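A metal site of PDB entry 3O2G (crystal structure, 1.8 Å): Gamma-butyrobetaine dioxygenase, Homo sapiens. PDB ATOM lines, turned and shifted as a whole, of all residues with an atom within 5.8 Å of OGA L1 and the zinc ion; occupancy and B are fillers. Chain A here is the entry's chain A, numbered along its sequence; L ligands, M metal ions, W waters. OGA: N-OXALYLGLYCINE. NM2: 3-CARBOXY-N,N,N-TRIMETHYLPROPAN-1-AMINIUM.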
ATOM      1  N   TRP A 182      -3.038  -3.363  30.945  1.00  0.00           N
ATOM      2  CA  TRP A 182      -4.175  -2.729  30.299  1.00  0.00           C
ATOM      3  C   TRP A 182      -4.558  -3.484  29.013  1.00  0.00           C
ATOM      4  O   TRP A 182      -3.700  -4.155  28.380  1.00  0.00           O
ATOM      5  CB  TRP A 182      -3.904  -1.256  30.020  1.00  0.00           C
ATOM      6  CG  TRP A 182      -2.459  -0.932  29.786  1.00  0.00           C
ATOM      7  CD1 TRP A 182      -1.577  -0.539  30.738  1.00  0.00           C
ATOM      8  CD2 TRP A 182      -1.721  -0.971  28.543  1.00  0.00           C
ATOM      9  NE1 TRP A 182      -0.331  -0.334  30.172  1.00  0.00           N
ATOM     10  CE2 TRP A 182      -0.383  -0.576  28.844  1.00  0.00           C
ATOM     11  CE3 TRP A 182      -2.044  -1.273  27.222  1.00  0.00           C
ATOM     12  CZ2 TRP A 182       0.607  -0.499  27.874  1.00  0.00           C
ATOM     13  CZ3 TRP A 182      -1.055  -1.196  26.252  1.00  0.00           C
ATOM     14  CH2 TRP A 182       0.272  -0.813  26.584  1.00  0.00           C
ATOM     15  N   VAL A 184      -5.977  -3.410  25.270  1.00  0.00           N
ATOM     16  CA  VAL A 184      -6.142  -2.618  24.078  1.00  0.00           C
ATOM     17  C   VAL A 184      -7.240  -3.278  23.257  1.00  0.00           C
ATOM     18  O   VAL A 184      -7.010  -4.300  22.634  1.00  0.00           O
ATOM     19  CB  VAL A 184      -4.841  -2.483  23.272  1.00  0.00           C
ATOM     20  CG1 VAL A 184      -5.087  -1.571  22.051  1.00  0.00           C
ATOM     21  CG2 VAL A 184      -3.691  -1.977  24.174  1.00  0.00           C
ATOM     22  N   ASN A 192      -9.259   6.799  25.848  1.00  0.00           N
ATOM     23  CA  ASN A 192      -7.969   6.927  25.173  1.00  0.00           C
ATOM     24  C   ASN A 192      -8.148   6.471  23.709  1.00  0.00           C
ATOM     25  O   ASN A 192      -8.900   5.540  23.458  1.00  0.00           O
ATOM     26  CB  ASN A 192      -6.899   6.075  25.902  1.00  0.00           C
ATOM     27  CG  ASN A 192      -5.458   6.396  25.456  1.00  0.00           C
ATOM     28  OD1 ASN A 192      -5.048   6.010  24.369  1.00  0.00           O
ATOM     29  ND2 ASN A 192      -4.672   7.074  26.324  1.00  0.00           N
ATOM     30  N   ALA A 194      -6.283   4.835  21.883  1.00  0.00           N
ATOM     31  CA  ALA A 194      -5.850   3.434  21.851  1.00  0.00           C
ATOM     32  C   ALA A 194      -7.038   2.445  21.925  1.00  0.00           C
ATOM     33  O   ALA A 194      -7.026   1.381  21.292  1.00  0.00           O
ATOM     34  CB  ALA A 194      -4.883   3.160  23.020  1.00  0.00           C
ATOM     35  N   TYR A 195      -8.062   2.795  22.709  1.00  0.00           N
ATOM     36  CA  TYR A 195      -9.172   1.911  22.996  1.00  0.00           C
ATOM     37  C   TYR A 195     -10.326   2.148  22.015  1.00  0.00           C
ATOM     38  O   TYR A 195     -11.476   2.141  22.396  1.00  0.00           O
ATOM     39  CB  TYR A 195      -9.634   2.082  24.430  1.00  0.00           C
ATOM     40  CG  TYR A 195      -8.544   1.831  25.478  1.00  0.00           C
ATOM     41  CD1 TYR A 195      -7.478   0.939  25.247  1.00  0.00           C
ATOM     42  CD2 TYR A 195      -8.575   2.477  26.705  1.00  0.00           C
ATOM     43  CE1 TYR A 195      -6.488   0.721  26.203  1.00  0.00           C
ATOM     44  CE2 TYR A 195      -7.569   2.278  27.661  1.00  0.00           C
ATOM     45  CZ  TYR A 195      -6.564   1.368  27.406  1.00  0.00           C
ATOM     46  OH  TYR A 195      -5.561   1.096  28.320  1.00  0.00           O
ATOM     47  N   LEU A 200      -3.502   4.429  14.784  1.00  0.00           N
ATOM     48  CA  LEU A 200      -2.562   5.130  15.628  1.00  0.00           C
ATOM     49  C   LEU A 200      -1.352   5.366  14.758  1.00  0.00           C
ATOM     50  O   LEU A 200      -0.741   4.385  14.235  1.00  0.00           O
ATOM     51  CB  LEU A 200      -2.215   4.287  16.855  1.00  0.00           C
ATOM     52  CG  LEU A 200      -3.381   3.832  17.755  1.00  0.00           C
ATOM     53  CD1 LEU A 200      -2.840   3.085  18.982  1.00  0.00           C
ATOM     54  CD2 LEU A 200      -4.247   5.071  18.152  1.00  0.00           C
ATOM     55  N   HIS A 203       3.873   6.966  17.498  1.00  0.00           N
ATOM     56  CA  HIS A 203       3.893   7.611  18.791  1.00  0.00           C
ATOM     57  C   HIS A 203       4.811   6.847  19.735  1.00  0.00           C
ATOM     58  O   HIS A 203       5.130   5.693  19.499  1.00  0.00           O
ATOM     59  CB  HIS A 203       2.503   7.690  19.443  1.00  0.00           C
ATOM     60  CG  HIS A 203       1.884   6.364  19.763  1.00  0.00           C
ATOM     61  ND1 HIS A 203       1.368   5.547  18.801  1.00  0.00           N
ATOM     62  CD2 HIS A 203       1.735   5.712  20.948  1.00  0.00           C
ATOM     63  CE1 HIS A 203       0.895   4.440  19.370  1.00  0.00           C
ATOM     64  NE2 HIS A 203       1.105   4.516  20.675  1.00  0.00           N
ATOM     65  N   THR A 204       5.212   7.522  20.803  1.00  0.00           N
ATOM     66  CA  THR A 204       5.704   6.910  22.040  1.00  0.00           C
ATOM     67  C   THR A 204       4.516   6.909  23.025  1.00  0.00           C
ATOM     68  O   THR A 204       3.664   7.761  22.946  1.00  0.00           O
ATOM     69  CB  THR A 204       6.942   7.686  22.624  1.00  0.00           C
ATOM     70  OG1 THR A 204       6.576   9.023  22.974  1.00  0.00           O
ATOM     71  CG2 THR A 204       8.082   7.729  21.609  1.00  0.00           C
ATOM     72  N   ASP A 205       4.461   5.930  23.931  1.00  0.00           N
ATOM     73  CA  ASP A 205       3.439   5.854  24.928  1.00  0.00           C
ATOM     74  C   ASP A 205       3.781   6.776  26.069  1.00  0.00           C
ATOM     75  O   ASP A 205       4.903   6.828  26.572  1.00  0.00           O
ATOM     76  CB  ASP A 205       3.275   4.418  25.453  1.00  0.00           C
ATOM     77  CG  ASP A 205       2.247   3.636  24.689  1.00  0.00           C
ATOM     78  OD1 ASP A 205       2.116   3.904  23.508  1.00  0.00           O
ATOM     79  OD2 ASP A 205       1.548   2.800  25.319  1.00  0.00           O
ATOM     80  N   GLN A 216       8.055  -1.137  26.920  1.00  0.00           N
ATOM     81  CA  GLN A 216       6.672  -1.520  26.717  1.00  0.00           C
ATOM     82  C   GLN A 216       6.593  -3.014  26.343  1.00  0.00           C
ATOM     83  O   GLN A 216       7.400  -3.517  25.568  1.00  0.00           O
ATOM     84  CB  GLN A 216       6.041  -0.661  25.626  1.00  0.00           C
ATOM     85  CG  GLN A 216       4.587  -0.933  25.449  1.00  0.00           C
ATOM     86  CD  GLN A 216       3.934  -0.098  24.374  1.00  0.00           C
ATOM     87  OE1 GLN A 216       2.959  -0.535  23.802  1.00  0.00           O
ATOM     88  NE2 GLN A 216       4.441   1.141  24.135  1.00  0.00           N
ATOM     89  N   LEU A 218       3.720  -5.751  24.842  1.00  0.00           N
ATOM     90  CA  LEU A 218       2.407  -5.836  24.179  1.00  0.00           C
ATOM     91  C   LEU A 218       2.189  -7.258  23.678  1.00  0.00           C
ATOM     92  O   LEU A 218       2.940  -7.765  22.853  1.00  0.00           O
ATOM     93  CB  LEU A 218       2.273  -4.876  23.007  1.00  0.00           C
ATOM     94  CG  LEU A 218       1.802  -3.425  23.127  1.00  0.00           C
ATOM     95  CD1 LEU A 218       1.776  -2.787  21.703  1.00  0.00           C
ATOM     96  CD2 LEU A 218       0.473  -3.220  23.816  1.00  0.00           C
ATOM     97  N   GLY A 228      -5.311  -3.645  11.649  1.00  0.00           N
ATOM     98  CA  GLY A 228      -4.607  -3.807  12.892  1.00  0.00           C
ATOM     99  C   GLY A 228      -3.156  -4.245  12.829  1.00  0.00           C
ATOM    100  O   GLY A 228      -2.613  -4.738  13.828  1.00  0.00           O
ATOM    101  N   ASP A 229      -2.541  -4.100  11.657  1.00  0.00           N
ATOM    102  CA  ASP A 229      -1.108  -4.341  11.533  1.00  0.00           C
ATOM    103  C   ASP A 229      -0.326  -3.344  12.377  1.00  0.00           C
ATOM    104  O   ASP A 229      -0.785  -2.214  12.641  1.00  0.00           O
ATOM    105  CB  ASP A 229      -0.652  -4.236  10.073  1.00  0.00           C
ATOM    106  CG  ASP A 229      -1.384  -5.184   9.161  1.00  0.00           C
ATOM    107  OD1 ASP A 229      -2.627  -5.044   9.008  1.00  0.00           O
ATOM    108  OD2 ASP A 229      -0.723  -6.058   8.560  1.00  0.00           O
ATOM    109  N   SER A 230       0.840  -3.776  12.813  1.00  0.00           N
ATOM    110  CA  SER A 230       1.743  -2.988  13.649  1.00  0.00           C
ATOM    111  C   SER A 230       2.800  -2.340  12.743  1.00  0.00           C
ATOM    112  O   SER A 230       3.144  -2.864  11.691  1.00  0.00           O
ATOM    113  CB  SER A 230       2.424  -3.907  14.659  1.00  0.00           C
ATOM    114  OG  SER A 230       1.506  -4.492  15.563  1.00  0.00           O
ATOM    115  N   MET A 333       0.876  -8.784  14.304  1.00  0.00           N
ATOM    116  CA  MET A 333       0.896  -9.688  15.464  1.00  0.00           C
ATOM    117  C   MET A 333      -0.155 -10.770  15.341  1.00  0.00           C
ATOM    118  O   MET A 333      -1.274 -10.499  14.878  1.00  0.00           O
ATOM    119  CB  MET A 333       0.662  -8.918  16.767  1.00  0.00           C
ATOM    120  CG  MET A 333       1.720  -7.831  17.032  1.00  0.00           C
ATOM    121  SD  MET A 333       1.682  -7.174  18.700  1.00  0.00           S
ATOM    122  CE  MET A 333       2.345  -8.539  19.632  1.00  0.00           C
ATOM    123  N   HIS A 348       5.882   3.622  17.552  1.00  0.00           N
ATOM    124  CA  HIS A 348       5.051   2.488  17.117  1.00  0.00           C
ATOM    125  C   HIS A 348       3.681   2.996  16.733  1.00  0.00           C
ATOM    126  O   HIS A 348       3.281   4.129  17.080  1.00  0.00           O
ATOM    127  CB  HIS A 348       4.977   1.395  18.177  1.00  0.00           C
ATOM    128  CG  HIS A 348       4.363   1.841  19.454  1.00  0.00           C
ATOM    129  ND1 HIS A 348       4.990   2.731  20.316  1.00  0.00           N
ATOM    130  CD2 HIS A 348       3.126   1.613  19.976  1.00  0.00           C
ATOM    131  CE1 HIS A 348       4.180   2.984  21.340  1.00  0.00           C
ATOM    132  NE2 HIS A 348       3.047   2.327  21.157  1.00  0.00           N
ATOM    133  N   GLY A 349       2.989   2.181  15.958  1.00  0.00           N
ATOM    134  CA  GLY A 349       1.667   2.553  15.485  1.00  0.00           C
ATOM    135  C   GLY A 349       0.867   1.333  15.096  1.00  0.00           C
ATOM    136  O   GLY A 349       1.382   0.180  15.102  1.00  0.00           O
ATOM    137  N   ARG A 350      -0.383   1.578  14.736  1.00  0.00           N
ATOM    138  CA  ARG A 350      -1.214   0.498  14.268  1.00  0.00           C
ATOM    139  C   ARG A 350      -2.216   0.987  13.223  1.00  0.00           C
ATOM    140  O   ARG A 350      -2.676   2.108  13.286  1.00  0.00           O
ATOM    141  CB  ARG A 350      -1.930  -0.183  15.408  1.00  0.00           C
ATOM    142  CG  ARG A 350      -2.946   0.616  16.117  1.00  0.00           C
ATOM    143  CD  ARG A 350      -4.254  -0.203  16.375  1.00  0.00           C
ATOM    144  NE  ARG A 350      -5.250   0.775  16.737  1.00  0.00           N
ATOM    145  CZ  ARG A 350      -5.733   1.041  17.961  1.00  0.00           C
ATOM    146  NH1 ARG A 350      -5.403   0.354  19.054  1.00  0.00           N
ATOM    147  NH2 ARG A 350      -6.612   2.029  18.072  1.00  0.00           N
ATOM    148  N   ARG A 361     -10.408  -7.942  18.410  1.00  0.00           N
ATOM    149  CA  ARG A 361      -8.991  -7.611  18.594  1.00  0.00           C
ATOM    150  C   ARG A 361      -8.761  -7.188  20.039  1.00  0.00           C
ATOM    151  O   ARG A 361      -9.525  -6.388  20.580  1.00  0.00           O
ATOM    152  CB  ARG A 361      -8.542  -6.489  17.627  1.00  0.00           C
ATOM    153  CG  ARG A 361      -7.024  -6.305  17.541  1.00  0.00           C
ATOM    154  CD  ARG A 361      -6.704  -5.158  16.599  1.00  0.00           C
ATOM    155  NE  ARG A 361      -5.276  -4.966  16.329  1.00  0.00           N
ATOM    156  CZ  ARG A 361      -4.428  -4.249  17.058  1.00  0.00           C
ATOM    157  NH1 ARG A 361      -4.784  -3.660  18.195  1.00  0.00           N
ATOM    158  NH2 ARG A 361      -3.159  -4.141  16.656  1.00  0.00           N
ATOM    159  N   LEU A 363      -5.223  -6.743  22.686  1.00  0.00           N
ATOM    160  CA  LEU A 363      -3.879  -6.853  23.179  1.00  0.00           C
ATOM    161  C   LEU A 363      -3.866  -6.566  24.699  1.00  0.00           C
ATOM    162  O   LEU A 363      -4.654  -5.733  25.189  1.00  0.00           O
ATOM    163  CB  LEU A 363      -2.955  -5.876  22.459  1.00  0.00           C
ATOM    164  CG  LEU A 363      -3.154  -5.679  20.963  1.00  0.00           C
ATOM    165  CD1 LEU A 363      -2.129  -4.607  20.469  1.00  0.00           C
ATOM    166  CD2 LEU A 363      -3.041  -7.000  20.204  1.00  0.00           C
ATOM    167  N   TYR A 367       4.072  -1.858  31.171  1.00  0.00           N
ATOM    168  CA  TYR A 367       5.309  -1.091  31.114  1.00  0.00           C
ATOM    169  C   TYR A 367       6.300  -1.555  32.171  1.00  0.00           C
ATOM    170  O   TYR A 367       5.922  -2.153  33.187  1.00  0.00           O
ATOM    171  CB  TYR A 367       5.005   0.398  31.361  1.00  0.00           C
ATOM    172  CG  TYR A 367       4.004   1.054  30.397  1.00  0.00           C
ATOM    173  CD1 TYR A 367       4.259   1.173  29.033  1.00  0.00           C
ATOM    174  CD2 TYR A 367       2.832   1.631  30.884  1.00  0.00           C
ATOM    175  CE1 TYR A 367       3.363   1.807  28.169  1.00  0.00           C
ATOM    176  CE2 TYR A 367       1.934   2.285  30.052  1.00  0.00           C
ATOM    177  CZ  TYR A 367       2.208   2.376  28.673  1.00  0.00           C
ATOM    178  OH  TYR A 367       1.305   2.990  27.804  1.00  0.00           O
HETATM  179  C1  OGA L   1      -1.452   1.882  22.214  1.00  0.00           C
HETATM  180  C2  OGA L   1      -0.875   1.143  21.032  1.00  0.00           C
HETATM  181  C4  OGA L   1      -0.923  -0.618  19.406  1.00  0.00           C
HETATM  182  C5  OGA L   1      -1.956  -1.580  18.790  1.00  0.00           C
HETATM  183  O1  OGA L   1      -2.456   1.361  22.755  1.00  0.00           O
HETATM  184  O2  OGA L   1      -0.871   2.953  22.580  1.00  0.00           O
HETATM  185  O2' OGA L   1       0.153   1.592  20.515  1.00  0.00           O
HETATM  186  O3  OGA L   1      -3.131  -1.445  19.180  1.00  0.00           O
HETATM  187  N1  OGA L   1      -1.514   0.074  20.559  1.00  0.00           N
HETATM  188  O4  OGA L   1      -1.508  -2.429  17.995  1.00  0.00           O
HETATM  189  N1  NM2 L   2      -2.390   3.192  26.919  1.00  0.00           N
HETATM  190  C8  NM2 L   2      -1.952   2.606  28.223  1.00  0.00           C
HETATM  191  O4  NM2 L   2      -1.734   7.484  26.057  1.00  0.00           O
HETATM  192  C5  NM2 L   2      -0.519   7.400  25.728  1.00  0.00           C
HETATM  193  O7  NM2 L   2       0.352   8.260  25.573  1.00  0.00           O
HETATM  194  C6  NM2 L   2      -0.631   6.048  25.039  1.00  0.00           C
HETATM  195  C2  NM2 L   2      -1.468   4.310  26.624  1.00  0.00           C
HETATM  196  C9  NM2 L   2      -3.770   3.724  26.907  1.00  0.00           C
HETATM  197  C10 NM2 L   2      -2.315   2.149  25.879  1.00  0.00           C
HETATM  198  C3  NM2 L   2      -1.504   5.006  25.296  1.00  0.00           C
HETATM  199 ZN    ZN M   1       1.129   2.843  21.929  1.00  0.00          ZN
HETATM  200  O   HOH W   1       1.057   1.151  23.178  1.00  0.00           O
HETATM  201  O   HOH W   2      -1.897   5.717  21.556  1.00  0.00           O
HETATM  202  O   HOH W   3       1.009  -2.346  17.147  1.00  0.00           O
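The side-chain amide nitrogen (ND2) of Asn 192 is in hydrogen-bond range of an oxygen (O4) of NM2 L2. The guanidinium group of Arg 361 is in salt-bridge range of an oxygen (O4) of OGA L1 (2.7 Å). The guanidinium group (NH1) of Arg 350 is in salt-bridge range of an oxygen (O3) of OGA L1 (2.9 Å).
The zinc ion is bound by a ring nitrogen (NE2) of His 203 (2.1 Å), water W1 (2.1 Å), an oxygen (O2) of OGA L1 (2.1 Å), an oxygen (O2') of OGA L1 (2.1 Å), a ring nitrogen (NE2) of His 348 (2.1 Å) and the side-chain carboxylate of Asp 205 (2.1 Å). The zinc ion has six donor atoms within binding distance.
Within 4 Å of the zinc ion: His 203, Asp 205 and His 348.
The side-chain carboxylate (OD2) of Asp 205 is in hydrogen-bond range of the side-chain hydroxyl (OH) of Tyr 367 (2.5 Å). N of Ala 194 sits at hydrogen-bond distance from OD1 of Asn 192 (3.0 Å). NE2 of His 348 lies close to NE2 of Gln 216 (3.5 Å). The guanidinium group (NH2) of Arg 361 lies within hydrogen-bond range of the backbone carbonyl oxygen (O) of Gly 228 (2.9 Å). O of Ala 194 sits at hydrogen-bond distance from NH1 of Arg 350, at 2.9 Å. The backbone carbonyl oxygen of Leu 363 lies within hydrogen-bond range of the backbone NH of Val 184 (2.7 Å). N of Arg 350 lies within hydrogen-bond range of O of Leu 200 (2.9 Å).
Val 184 touches OGA L1. CB of Ala 194 touches O1 of OGA L1, at 3.0 Å. Leu 200 touches OGA L1. Leu 363 touches OGA L1. Nine residues have an atom within 4 Å of OGA L1: Val 184, Ala 194, Leu 200, His 203, Asp 205, His 348, Arg 350, Arg 361 and Leu 363. The nearest printed residue that does not touch OGA L1 is Leu 218 (4.2 Å).
Water W1 lies within hydrogen-bond range of the side-chain amide oxygen (OE1) of Gln 216 (2.6 Å) and the side-chain carboxylate (OD2) of Asp 205 (2.7 Å). Water W3 lies within hydrogen-bond range of O4 of OGA L1 (2.7 Å), OG of Ser 230 (2.7 Å) and O of Gly 349 (3.3 Å).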
